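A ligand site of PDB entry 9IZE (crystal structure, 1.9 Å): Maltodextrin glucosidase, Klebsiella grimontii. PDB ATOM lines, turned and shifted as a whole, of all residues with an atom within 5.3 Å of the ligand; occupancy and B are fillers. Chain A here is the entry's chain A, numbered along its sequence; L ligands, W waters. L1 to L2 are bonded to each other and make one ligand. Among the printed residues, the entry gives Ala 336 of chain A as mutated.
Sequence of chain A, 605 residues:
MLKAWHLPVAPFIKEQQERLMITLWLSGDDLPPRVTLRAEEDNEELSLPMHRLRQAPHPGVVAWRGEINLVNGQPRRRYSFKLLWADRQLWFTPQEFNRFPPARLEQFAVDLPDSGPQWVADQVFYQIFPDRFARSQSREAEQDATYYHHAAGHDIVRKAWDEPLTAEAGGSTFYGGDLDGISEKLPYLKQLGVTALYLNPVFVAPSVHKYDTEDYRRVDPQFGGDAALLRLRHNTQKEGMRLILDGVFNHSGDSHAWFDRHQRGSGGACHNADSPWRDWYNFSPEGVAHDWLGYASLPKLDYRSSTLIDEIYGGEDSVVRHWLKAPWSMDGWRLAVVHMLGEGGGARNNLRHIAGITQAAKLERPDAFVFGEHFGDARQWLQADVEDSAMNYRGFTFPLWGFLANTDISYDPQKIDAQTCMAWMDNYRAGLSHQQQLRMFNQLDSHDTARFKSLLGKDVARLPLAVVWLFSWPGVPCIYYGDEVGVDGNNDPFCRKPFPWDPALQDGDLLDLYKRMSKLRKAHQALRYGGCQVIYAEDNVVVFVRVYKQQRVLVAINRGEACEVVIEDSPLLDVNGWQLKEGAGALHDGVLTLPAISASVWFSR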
ATOM      1  N   PHE A 129      20.296 -18.264 -16.890  1.00  0.00           N
ATOM      2  CA  PHE A 129      21.319 -18.441 -15.861  1.00  0.00           C
ATOM      3  C   PHE A 129      22.601 -17.843 -16.443  1.00  0.00           C
ATOM      4  O   PHE A 129      23.248 -18.482 -17.280  1.00  0.00           O
ATOM      5  CB  PHE A 129      21.462 -19.934 -15.525  1.00  0.00           C
ATOM      6  CG  PHE A 129      22.309 -20.230 -14.314  1.00  0.00           C
ATOM      7  CD1 PHE A 129      21.741 -20.311 -13.046  1.00  0.00           C
ATOM      8  CD2 PHE A 129      23.662 -20.485 -14.453  1.00  0.00           C
ATOM      9  CE1 PHE A 129      22.517 -20.608 -11.937  1.00  0.00           C
ATOM     10  CE2 PHE A 129      24.451 -20.788 -13.355  1.00  0.00           C
ATOM     11  CZ  PHE A 129      23.872 -20.847 -12.091  1.00  0.00           C
ATOM     12  N   GLY A 170      30.229 -27.519  -7.846  1.00  0.00           N
ATOM     13  CA  GLY A 170      29.066 -27.129  -8.621  1.00  0.00           C
ATOM     14  C   GLY A 170      28.730 -25.655  -8.500  1.00  0.00           C
ATOM     15  O   GLY A 170      28.261 -25.038  -9.459  1.00  0.00           O
ATOM     16  N   GLY A 171      28.944 -25.075  -7.317  1.00  0.00           N
ATOM     17  CA  GLY A 171      28.705 -23.676  -7.054  1.00  0.00           C
ATOM     18  C   GLY A 171      29.881 -22.758  -7.312  1.00  0.00           C
ATOM     19  O   GLY A 171      29.774 -21.553  -7.068  1.00  0.00           O
ATOM     20  N   HIS A 209      26.100 -19.210  -9.111  1.00  0.00           N
ATOM     21  CA  HIS A 209      24.656 -18.954  -9.174  1.00  0.00           C
ATOM     22  C   HIS A 209      24.291 -17.625  -8.527  1.00  0.00           C
ATOM     23  O   HIS A 209      23.265 -17.026  -8.900  1.00  0.00           O
ATOM     24  CB  HIS A 209      23.890 -20.084  -8.485  1.00  0.00           C
ATOM     25  CG  HIS A 209      24.391 -20.399  -7.119  1.00  0.00           C
ATOM     26  ND1 HIS A 209      24.146 -19.599  -6.023  1.00  0.00           N
ATOM     27  CD2 HIS A 209      25.169 -21.415  -6.672  1.00  0.00           C
ATOM     28  CE1 HIS A 209      24.724 -20.115  -4.960  1.00  0.00           C
ATOM     29  NE2 HIS A 209      25.363 -21.219  -5.327  1.00  0.00           N
ATOM     30  N   TYR A 211      23.128 -16.724  -5.569  1.00  0.00           N
ATOM     31  CA  TYR A 211      22.099 -16.586  -4.532  1.00  0.00           C
ATOM     32  C   TYR A 211      22.714 -16.276  -3.171  1.00  0.00           C
ATOM     33  O   TYR A 211      21.972 -16.025  -2.210  1.00  0.00           O
ATOM     34  CB  TYR A 211      21.249 -17.844  -4.475  1.00  0.00           C
ATOM     35  CG  TYR A 211      20.302 -17.953  -5.635  1.00  0.00           C
ATOM     36  CD1 TYR A 211      19.109 -17.226  -5.651  1.00  0.00           C
ATOM     37  CD2 TYR A 211      20.597 -18.748  -6.729  1.00  0.00           C
ATOM     38  CE1 TYR A 211      18.226 -17.304  -6.731  1.00  0.00           C
ATOM     39  CE2 TYR A 211      19.727 -18.831  -7.820  1.00  0.00           C
ATOM     40  CZ  TYR A 211      18.550 -18.111  -7.815  1.00  0.00           C
ATOM     41  OH  TYR A 211      17.685 -18.205  -8.876  1.00  0.00           O
ATOM     42  N   VAL A 248      16.572 -11.928  -3.957  1.00  0.00           N
ATOM     43  CA  VAL A 248      16.894 -12.939  -2.962  1.00  0.00           C
ATOM     44  C   VAL A 248      16.905 -12.288  -1.593  1.00  0.00           C
ATOM     45  O   VAL A 248      17.948 -11.807  -1.121  1.00  0.00           O
ATOM     46  CB  VAL A 248      18.228 -13.627  -3.296  1.00  0.00           C
ATOM     47  CG1 VAL A 248      18.417 -14.891  -2.469  1.00  0.00           C
ATOM     48  CG2 VAL A 248      18.281 -13.961  -4.780  1.00  0.00           C
ATOM     49  N   HIS A 251      17.268 -14.511   2.588  1.00  0.00           N
ATOM     50  CA  HIS A 251      18.597 -14.668   3.159  1.00  0.00           C
ATOM     51  C   HIS A 251      19.563 -13.841   2.334  1.00  0.00           C
ATOM     52  O   HIS A 251      19.283 -13.497   1.184  1.00  0.00           O
ATOM     53  CB  HIS A 251      19.011 -16.134   3.153  1.00  0.00           C
ATOM     54  CG  HIS A 251      18.935 -16.787   1.804  1.00  0.00           C
ATOM     55  ND1 HIS A 251      17.856 -17.533   1.396  1.00  0.00           N
ATOM     56  CD2 HIS A 251      19.816 -16.805   0.775  1.00  0.00           C
ATOM     57  CE1 HIS A 251      18.075 -17.999   0.175  1.00  0.00           C
ATOM     58  NE2 HIS A 251      19.255 -17.564  -0.228  1.00  0.00           N
ATOM     59  N   TRP A 292      19.417 -20.936   5.231  1.00  0.00           N
ATOM     60  CA  TRP A 292      18.506 -21.568   4.278  1.00  0.00           C
ATOM     61  C   TRP A 292      18.790 -23.055   4.262  1.00  0.00           C
ATOM     62  O   TRP A 292      19.784 -23.514   3.703  1.00  0.00           O
ATOM     63  CB  TRP A 292      18.635 -20.961   2.883  1.00  0.00           C
ATOM     64  CG  TRP A 292      17.666 -21.569   1.906  1.00  0.00           C
ATOM     65  CD1 TRP A 292      16.328 -21.292   1.817  1.00  0.00           C
ATOM     66  CD2 TRP A 292      17.940 -22.549   0.898  1.00  0.00           C
ATOM     67  NE1 TRP A 292      15.758 -22.038   0.807  1.00  0.00           N
ATOM     68  CE2 TRP A 292      16.726 -22.814   0.227  1.00  0.00           C
ATOM     69  CE3 TRP A 292      19.094 -23.229   0.490  1.00  0.00           C
ATOM     70  CZ2 TRP A 292      16.629 -23.730  -0.826  1.00  0.00           C
ATOM     71  CZ3 TRP A 292      19.006 -24.136  -0.558  1.00  0.00           C
ATOM     72  CH2 TRP A 292      17.776 -24.380  -1.202  1.00  0.00           C
ATOM     73  N   TYR A 295      22.417 -24.415   4.860  1.00  0.00           N
ATOM     74  CA  TYR A 295      23.576 -23.967   4.099  1.00  0.00           C
ATOM     75  C   TYR A 295      24.134 -22.727   4.787  1.00  0.00           C
ATOM     76  O   TYR A 295      23.504 -21.658   4.760  1.00  0.00           O
ATOM     77  CB  TYR A 295      23.197 -23.713   2.644  1.00  0.00           C
ATOM     78  CG  TYR A 295      22.871 -24.994   1.874  1.00  0.00           C
ATOM     79  CD1 TYR A 295      23.868 -25.726   1.241  1.00  0.00           C
ATOM     80  CD2 TYR A 295      21.565 -25.479   1.797  1.00  0.00           C
ATOM     81  CE1 TYR A 295      23.586 -26.901   0.542  1.00  0.00           C
ATOM     82  CE2 TYR A 295      21.271 -26.658   1.106  1.00  0.00           C
ATOM     83  CZ  TYR A 295      22.285 -27.361   0.488  1.00  0.00           C
ATOM     84  OH  TYR A 295      21.979 -28.521  -0.199  1.00  0.00           O
ATOM     85  N   LEU A 298      24.218 -19.125   3.455  1.00  0.00           N
ATOM     86  CA  LEU A 298      22.961 -18.423   3.198  1.00  0.00           C
ATOM     87  C   LEU A 298      22.269 -18.083   4.509  1.00  0.00           C
ATOM     88  O   LEU A 298      21.229 -18.662   4.850  1.00  0.00           O
ATOM     89  CB  LEU A 298      22.068 -19.262   2.287  1.00  0.00           C
ATOM     90  CG  LEU A 298      22.724 -19.689   0.968  1.00  0.00           C
ATOM     91  CD1 LEU A 298      21.869 -20.683   0.199  1.00  0.00           C
ATOM     92  CD2 LEU A 298      23.035 -18.474   0.096  1.00  0.00           C
ATOM     93  N   ARG A 334      11.511 -11.593  -9.447  1.00  0.00           N
ATOM     94  CA  ARG A 334      11.228 -12.976  -9.093  1.00  0.00           C
ATOM     95  C   ARG A 334      11.721 -13.168  -7.658  1.00  0.00           C
ATOM     96  O   ARG A 334      12.902 -12.933  -7.376  1.00  0.00           O
ATOM     97  CB  ARG A 334      11.905 -13.931 -10.081  1.00  0.00           C
ATOM     98  CG  ARG A 334      11.776 -15.438  -9.812  1.00  0.00           C
ATOM     99  CD  ARG A 334      12.815 -15.946  -8.812  1.00  0.00           C
ATOM    100  NE  ARG A 334      12.885 -17.399  -8.779  1.00  0.00           N
ATOM    101  CZ  ARG A 334      13.773 -18.085  -8.062  1.00  0.00           C
ATOM    102  NH1 ARG A 334      14.674 -17.465  -7.311  1.00  0.00           N
ATOM    103  NH2 ARG A 334      13.751 -19.411  -8.106  1.00  0.00           N
ATOM    104  N   ALA A 336      12.973 -15.126  -4.743  1.00  0.00           N
ATOM    105  CA  ALA A 336      13.560 -16.389  -4.320  1.00  0.00           C
ATOM    106  C   ALA A 336      13.066 -16.757  -2.922  1.00  0.00           C
ATOM    107  O   ALA A 336      13.042 -15.916  -2.019  1.00  0.00           O
ATOM    108  CB  ALA A 336      15.077 -16.282  -4.319  1.00  0.00           C
ATOM    109  N   VAL A 337      12.694 -18.030  -2.749  1.00  0.00           N
ATOM    110  CA  VAL A 337      12.305 -18.567  -1.441  1.00  0.00           C
ATOM    111  C   VAL A 337      11.250 -17.674  -0.799  1.00  0.00           C
ATOM    112  O   VAL A 337      11.317 -17.360   0.394  1.00  0.00           O
ATOM    113  CB  VAL A 337      13.536 -18.732  -0.531  1.00  0.00           C
ATOM    114  CG1 VAL A 337      13.216 -19.677   0.652  1.00  0.00           C
ATOM    115  CG2 VAL A 337      14.702 -19.267  -1.328  1.00  0.00           C
ATOM    116  N   GLU A 373       8.880 -17.652  -6.122  1.00  0.00           N
ATOM    117  CA  GLU A 373       9.308 -19.037  -6.311  1.00  0.00           C
ATOM    118  C   GLU A 373       8.481 -19.944  -5.404  1.00  0.00           C
ATOM    119  O   GLU A 373       8.642 -19.909  -4.183  1.00  0.00           O
ATOM    120  CB  GLU A 373      10.785 -19.189  -5.972  1.00  0.00           C
ATOM    121  CG  GLU A 373      11.269 -20.616  -6.178  1.00  0.00           C
ATOM    122  CD  GLU A 373      12.579 -20.949  -5.483  1.00  0.00           C
ATOM    123  OE1 GLU A 373      12.979 -20.229  -4.537  1.00  0.00           O
ATOM    124  OE2 GLU A 373      13.202 -21.954  -5.890  1.00  0.00           O
ATOM    125  N   HIS A 447      16.473 -23.977 -13.479  1.00  0.00           N
ATOM    126  CA  HIS A 447      17.828 -24.181 -12.977  1.00  0.00           C
ATOM    127  C   HIS A 447      17.850 -25.000 -11.690  1.00  0.00           C
ATOM    128  O   HIS A 447      18.930 -25.313 -11.173  1.00  0.00           O
ATOM    129  CB  HIS A 447      18.493 -22.837 -12.740  1.00  0.00           C
ATOM    130  CG  HIS A 447      17.862 -22.043 -11.653  1.00  0.00           C
ATOM    131  ND1 HIS A 447      16.528 -21.695 -11.671  1.00  0.00           N
ATOM    132  CD2 HIS A 447      18.358 -21.556 -10.486  1.00  0.00           C
ATOM    133  CE1 HIS A 447      16.236 -21.008 -10.574  1.00  0.00           C
ATOM    134  NE2 HIS A 447      17.340 -20.908  -9.836  1.00  0.00           N
ATOM    135  N   ASP A 448      16.672 -25.332 -11.160  1.00  0.00           N
ATOM    136  CA  ASP A 448      16.551 -26.113  -9.929  1.00  0.00           C
ATOM    137  C   ASP A 448      15.917 -27.475 -10.167  1.00  0.00           C
ATOM    138  O   ASP A 448      15.529 -28.145  -9.194  1.00  0.00           O
ATOM    139  CB  ASP A 448      15.736 -25.334  -8.883  1.00  0.00           C
ATOM    140  CG  ASP A 448      16.464 -24.111  -8.333  1.00  0.00           C
ATOM    141  OD1 ASP A 448      17.723 -24.115  -8.250  1.00  0.00           O
ATOM    142  OD2 ASP A 448      15.767 -23.132  -7.961  1.00  0.00           O
ATOM    143  N   ASN A 491      19.426 -32.950 -12.609  1.00  0.00           N
ATOM    144  CA  ASN A 491      19.251 -31.780 -11.769  1.00  0.00           C
ATOM    145  C   ASN A 491      20.594 -31.138 -11.439  1.00  0.00           C
ATOM    146  O   ASN A 491      21.658 -31.764 -11.560  1.00  0.00           O
ATOM    147  CB  ASN A 491      18.514 -32.144 -10.480  1.00  0.00           C
ATOM    148  CG  ASN A 491      18.075 -30.924  -9.704  1.00  0.00           C
ATOM    149  OD1 ASN A 491      17.844 -29.862 -10.291  1.00  0.00           O
ATOM    150  ND2 ASN A 491      17.968 -31.049  -8.388  1.00  0.00           N
ATOM    151  N   ASP A 492      20.532 -29.853 -11.078  1.00  0.00           N
ATOM    152  CA  ASP A 492      21.578 -29.047 -10.468  1.00  0.00           C
ATOM    153  C   ASP A 492      22.641 -29.933  -9.829  1.00  0.00           C
ATOM    154  O   ASP A 492      22.346 -30.657  -8.860  1.00  0.00           O
ATOM    155  CB  ASP A 492      20.941 -28.122  -9.419  1.00  0.00           C
ATOM    156  CG  ASP A 492      21.930 -27.163  -8.802  1.00  0.00           C
ATOM    157  OD1 ASP A 492      23.058 -27.027  -9.310  1.00  0.00           O
ATOM    158  OD2 ASP A 492      21.564 -26.526  -7.793  1.00  0.00           O
ATOM    159  N   PRO A 493      23.899 -29.891 -10.306  1.00  0.00           N
ATOM    160  CA  PRO A 493      24.487 -28.919 -11.254  1.00  0.00           C
ATOM    161  C   PRO A 493      24.272 -29.209 -12.727  1.00  0.00           C
ATOM    162  O   PRO A 493      24.586 -28.350 -13.564  1.00  0.00           O
ATOM    163  CB  PRO A 493      25.982 -29.007 -10.908  1.00  0.00           C
ATOM    164  CG  PRO A 493      26.176 -30.482 -10.577  1.00  0.00           C
ATOM    165  CD  PRO A 493      24.893 -30.892  -9.867  1.00  0.00           C
ATOM    166  N   ARG A 496      22.439 -26.981 -15.842  1.00  0.00           N
ATOM    167  CA  ARG A 496      22.947 -25.639 -16.137  1.00  0.00           C
ATOM    168  C   ARG A 496      24.089 -25.678 -17.147  1.00  0.00           C
ATOM    169  O   ARG A 496      25.100 -25.005 -16.998  1.00  0.00           O
ATOM    170  CB  ARG A 496      23.370 -24.947 -14.848  1.00  0.00           C
ATOM    171  CG  ARG A 496      22.260 -24.920 -13.793  1.00  0.00           C
ATOM    172  CD  ARG A 496      22.755 -24.559 -12.403  1.00  0.00           C
ATOM    173  NE  ARG A 496      21.652 -24.541 -11.437  1.00  0.00           N
ATOM    174  CZ  ARG A 496      21.746 -24.069 -10.199  1.00  0.00           C
ATOM    175  NH1 ARG A 496      22.890 -23.590  -9.720  1.00  0.00           N
ATOM    176  NH2 ARG A 496      20.664 -24.049  -9.436  1.00  0.00           N
HETATM  177  C1  LIG L   1      16.648 -19.811  -4.936  1.00  0.00           C
HETATM  178  C2  LIG L   1      17.130 -20.531  -6.206  1.00  0.00           C
HETATM  179  C3  LIG L   1      17.967 -21.716  -5.923  1.00  0.00           C
HETATM  180  C4  LIG L   1      18.902 -21.442  -4.779  1.00  0.00           C
HETATM  181  C5  LIG L   1      18.080 -21.353  -3.492  1.00  0.00           C
HETATM  182  C6  LIG L   1      18.865 -20.869  -2.293  1.00  0.00           C
HETATM  183  O1  LIG L   1      15.299 -19.554  -4.915  1.00  0.00           O
HETATM  184  O2  LIG L   1      16.071 -20.857  -7.133  1.00  0.00           O
HETATM  185  O3  LIG L   1      18.678 -21.975  -7.188  1.00  0.00           O
HETATM  186  O4  LIG L   1      19.880 -22.503  -4.704  1.00  0.00           O
HETATM  187  O5  LIG L   1      16.974 -20.416  -3.617  1.00  0.00           O
HETATM  188  O6  LIG L   1      19.228 -19.518  -2.535  1.00  0.00           O
HETATM  189  O1  LG2 L   2      21.877 -22.217  -3.518  1.00  0.00           O
HETATM  190  C1  LG2 L   2      21.974 -22.606  -5.821  1.00  0.00           C
HETATM  191  C2  LG2 L   2      21.824 -24.057  -5.709  1.00  0.00           C
HETATM  192  C3  LG2 L   2      25.066 -26.676  -3.507  1.00  0.00           C
HETATM  193  C4  LG2 L   2      22.025 -29.735  -4.710  1.00  0.00           C
HETATM  194  C5  LG2 L   2      22.755 -28.603  -3.999  1.00  0.00           C
HETATM  195  C6  LG2 L   2      22.910 -27.224  -4.782  1.00  0.00           C
HETATM  196  C7  LG2 L   2      23.448 -26.305  -3.841  1.00  0.00           C
HETATM  197  C8  LG2 L   2      22.078 -24.600  -4.348  1.00  0.00           C
HETATM  198  C9  LG2 L   2      21.788 -23.660  -3.151  1.00  0.00           C
HETATM  199  C10 LG2 L   2      22.641 -23.817  -1.939  1.00  0.00           C
HETATM  200  C11 LG2 L   2      21.156 -21.922  -4.749  1.00  0.00           C
HETATM  201  C12 LG2 L   2      25.239 -27.967  -3.358  1.00  0.00           C
HETATM  202  C13 LG2 L   2      23.751 -28.800  -2.983  1.00  0.00           C
HETATM  203  N1  LG2 L   2      23.480 -25.045  -4.453  1.00  0.00           N
HETATM  204  O2  LG2 L   2      21.621 -29.090  -5.897  1.00  0.00           O
HETATM  205  O3  LG2 L   2      21.434 -22.299  -7.090  1.00  0.00           O
HETATM  206  O4  LG2 L   2      22.779 -24.606  -6.671  1.00  0.00           O
HETATM  207  O5  LG2 L   2      25.722 -26.037  -4.637  1.00  0.00           O
HETATM  208  O6  LG2 L   2      26.161 -28.105  -2.235  1.00  0.00           O
HETATM  209  O7  LG2 L   2      23.798 -30.155  -2.698  1.00  0.00           O
HETATM  210  O   HOH W   1      27.514 -28.877   0.346  1.00  0.00           O
HETATM  211  O   HOH W   2      18.660 -25.443  -4.526  1.00  0.00           O
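ND1 of His 209 is in hydrogen-bond range of N of Tyr 211, at 3.1 Å. The guanidinium group (NH1) of Arg 334 lies within hydrogen-bond range of the side-chain hydroxyl (OH) of Tyr 211 (3.5 Å). N of Trp 292 sits at hydrogen-bond distance from O of Leu 298 (2.9 Å). The side-chain carboxylate of Glu 373 sits at hydrogen-bond distance from the backbone NH of Val 337 (2.8 Å). The guanidinium group (NH2) of Arg 496 is in salt-bridge range of the side-chain carboxylate (OD1) of Asp 448, 3.2 Å away. OD2 of Asp 448 lies within hydrogen-bond range of NE2 of His 447 (3.3 Å). O of His 447 sits at hydrogen-bond distance from NH2 of Arg 496 (2.8 Å). The guanidinium group of Arg 496 lies within salt-bridge range of the side-chain carboxylate of Asp 492, at 3.1 Å.
The guanidinium group (NH2) of Arg 334 sits at hydrogen-bond distance from an oxygen (O2) of LIG L1. The side-chain hydroxyl (OH) of Tyr 295 sits close to an oxygen (O7) of LG2 L2. The side-chain carboxylate of Asp 492 lies within hydrogen-bond range of an oxygen (O4) of LG2 L2 (2.5 Å). A ring nitrogen (NE2) of His 447 is in hydrogen-bond range of an oxygen (O2) of LIG L1. O1 of LIG L1 sits at hydrogen-bond distance from OE1 of Glu 373 (2.4 Å). OD2 of Asp 448 is in hydrogen-bond range of O2 of LIG L1 (2.4 Å). An oxygen (O3) of LG2 L2 is in hydrogen-bond range of the guanidinium group (NH2) of Arg 496, 3.0 Å away. The backbone carbonyl oxygen (O) of Asp 492 lies within hydrogen-bond range of an oxygen (O2) of LG2 L2 (3.4 Å). NE2 of His 251 is in hydrogen-bond range of O6 of LIG L1 (3.0 Å).
Residues that only touch the ligand: His 209 (3.5 Å), Tyr 211 (3.2 Å), Trp 292 (3.7 Å), Leu 298 (3.9 Å), Ala 336 (3.3 Å) and Val 337 (3.4 Å). Hydrophobic or aromatic side chains within 4 Å of the ligand: His 209, Tyr 211, His 251, Trp 292, Tyr 295, Leu 298, Ala 336, Val 337 and His 447. Of the 20 residues printed, 14 come within 4 Å of the ligand.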
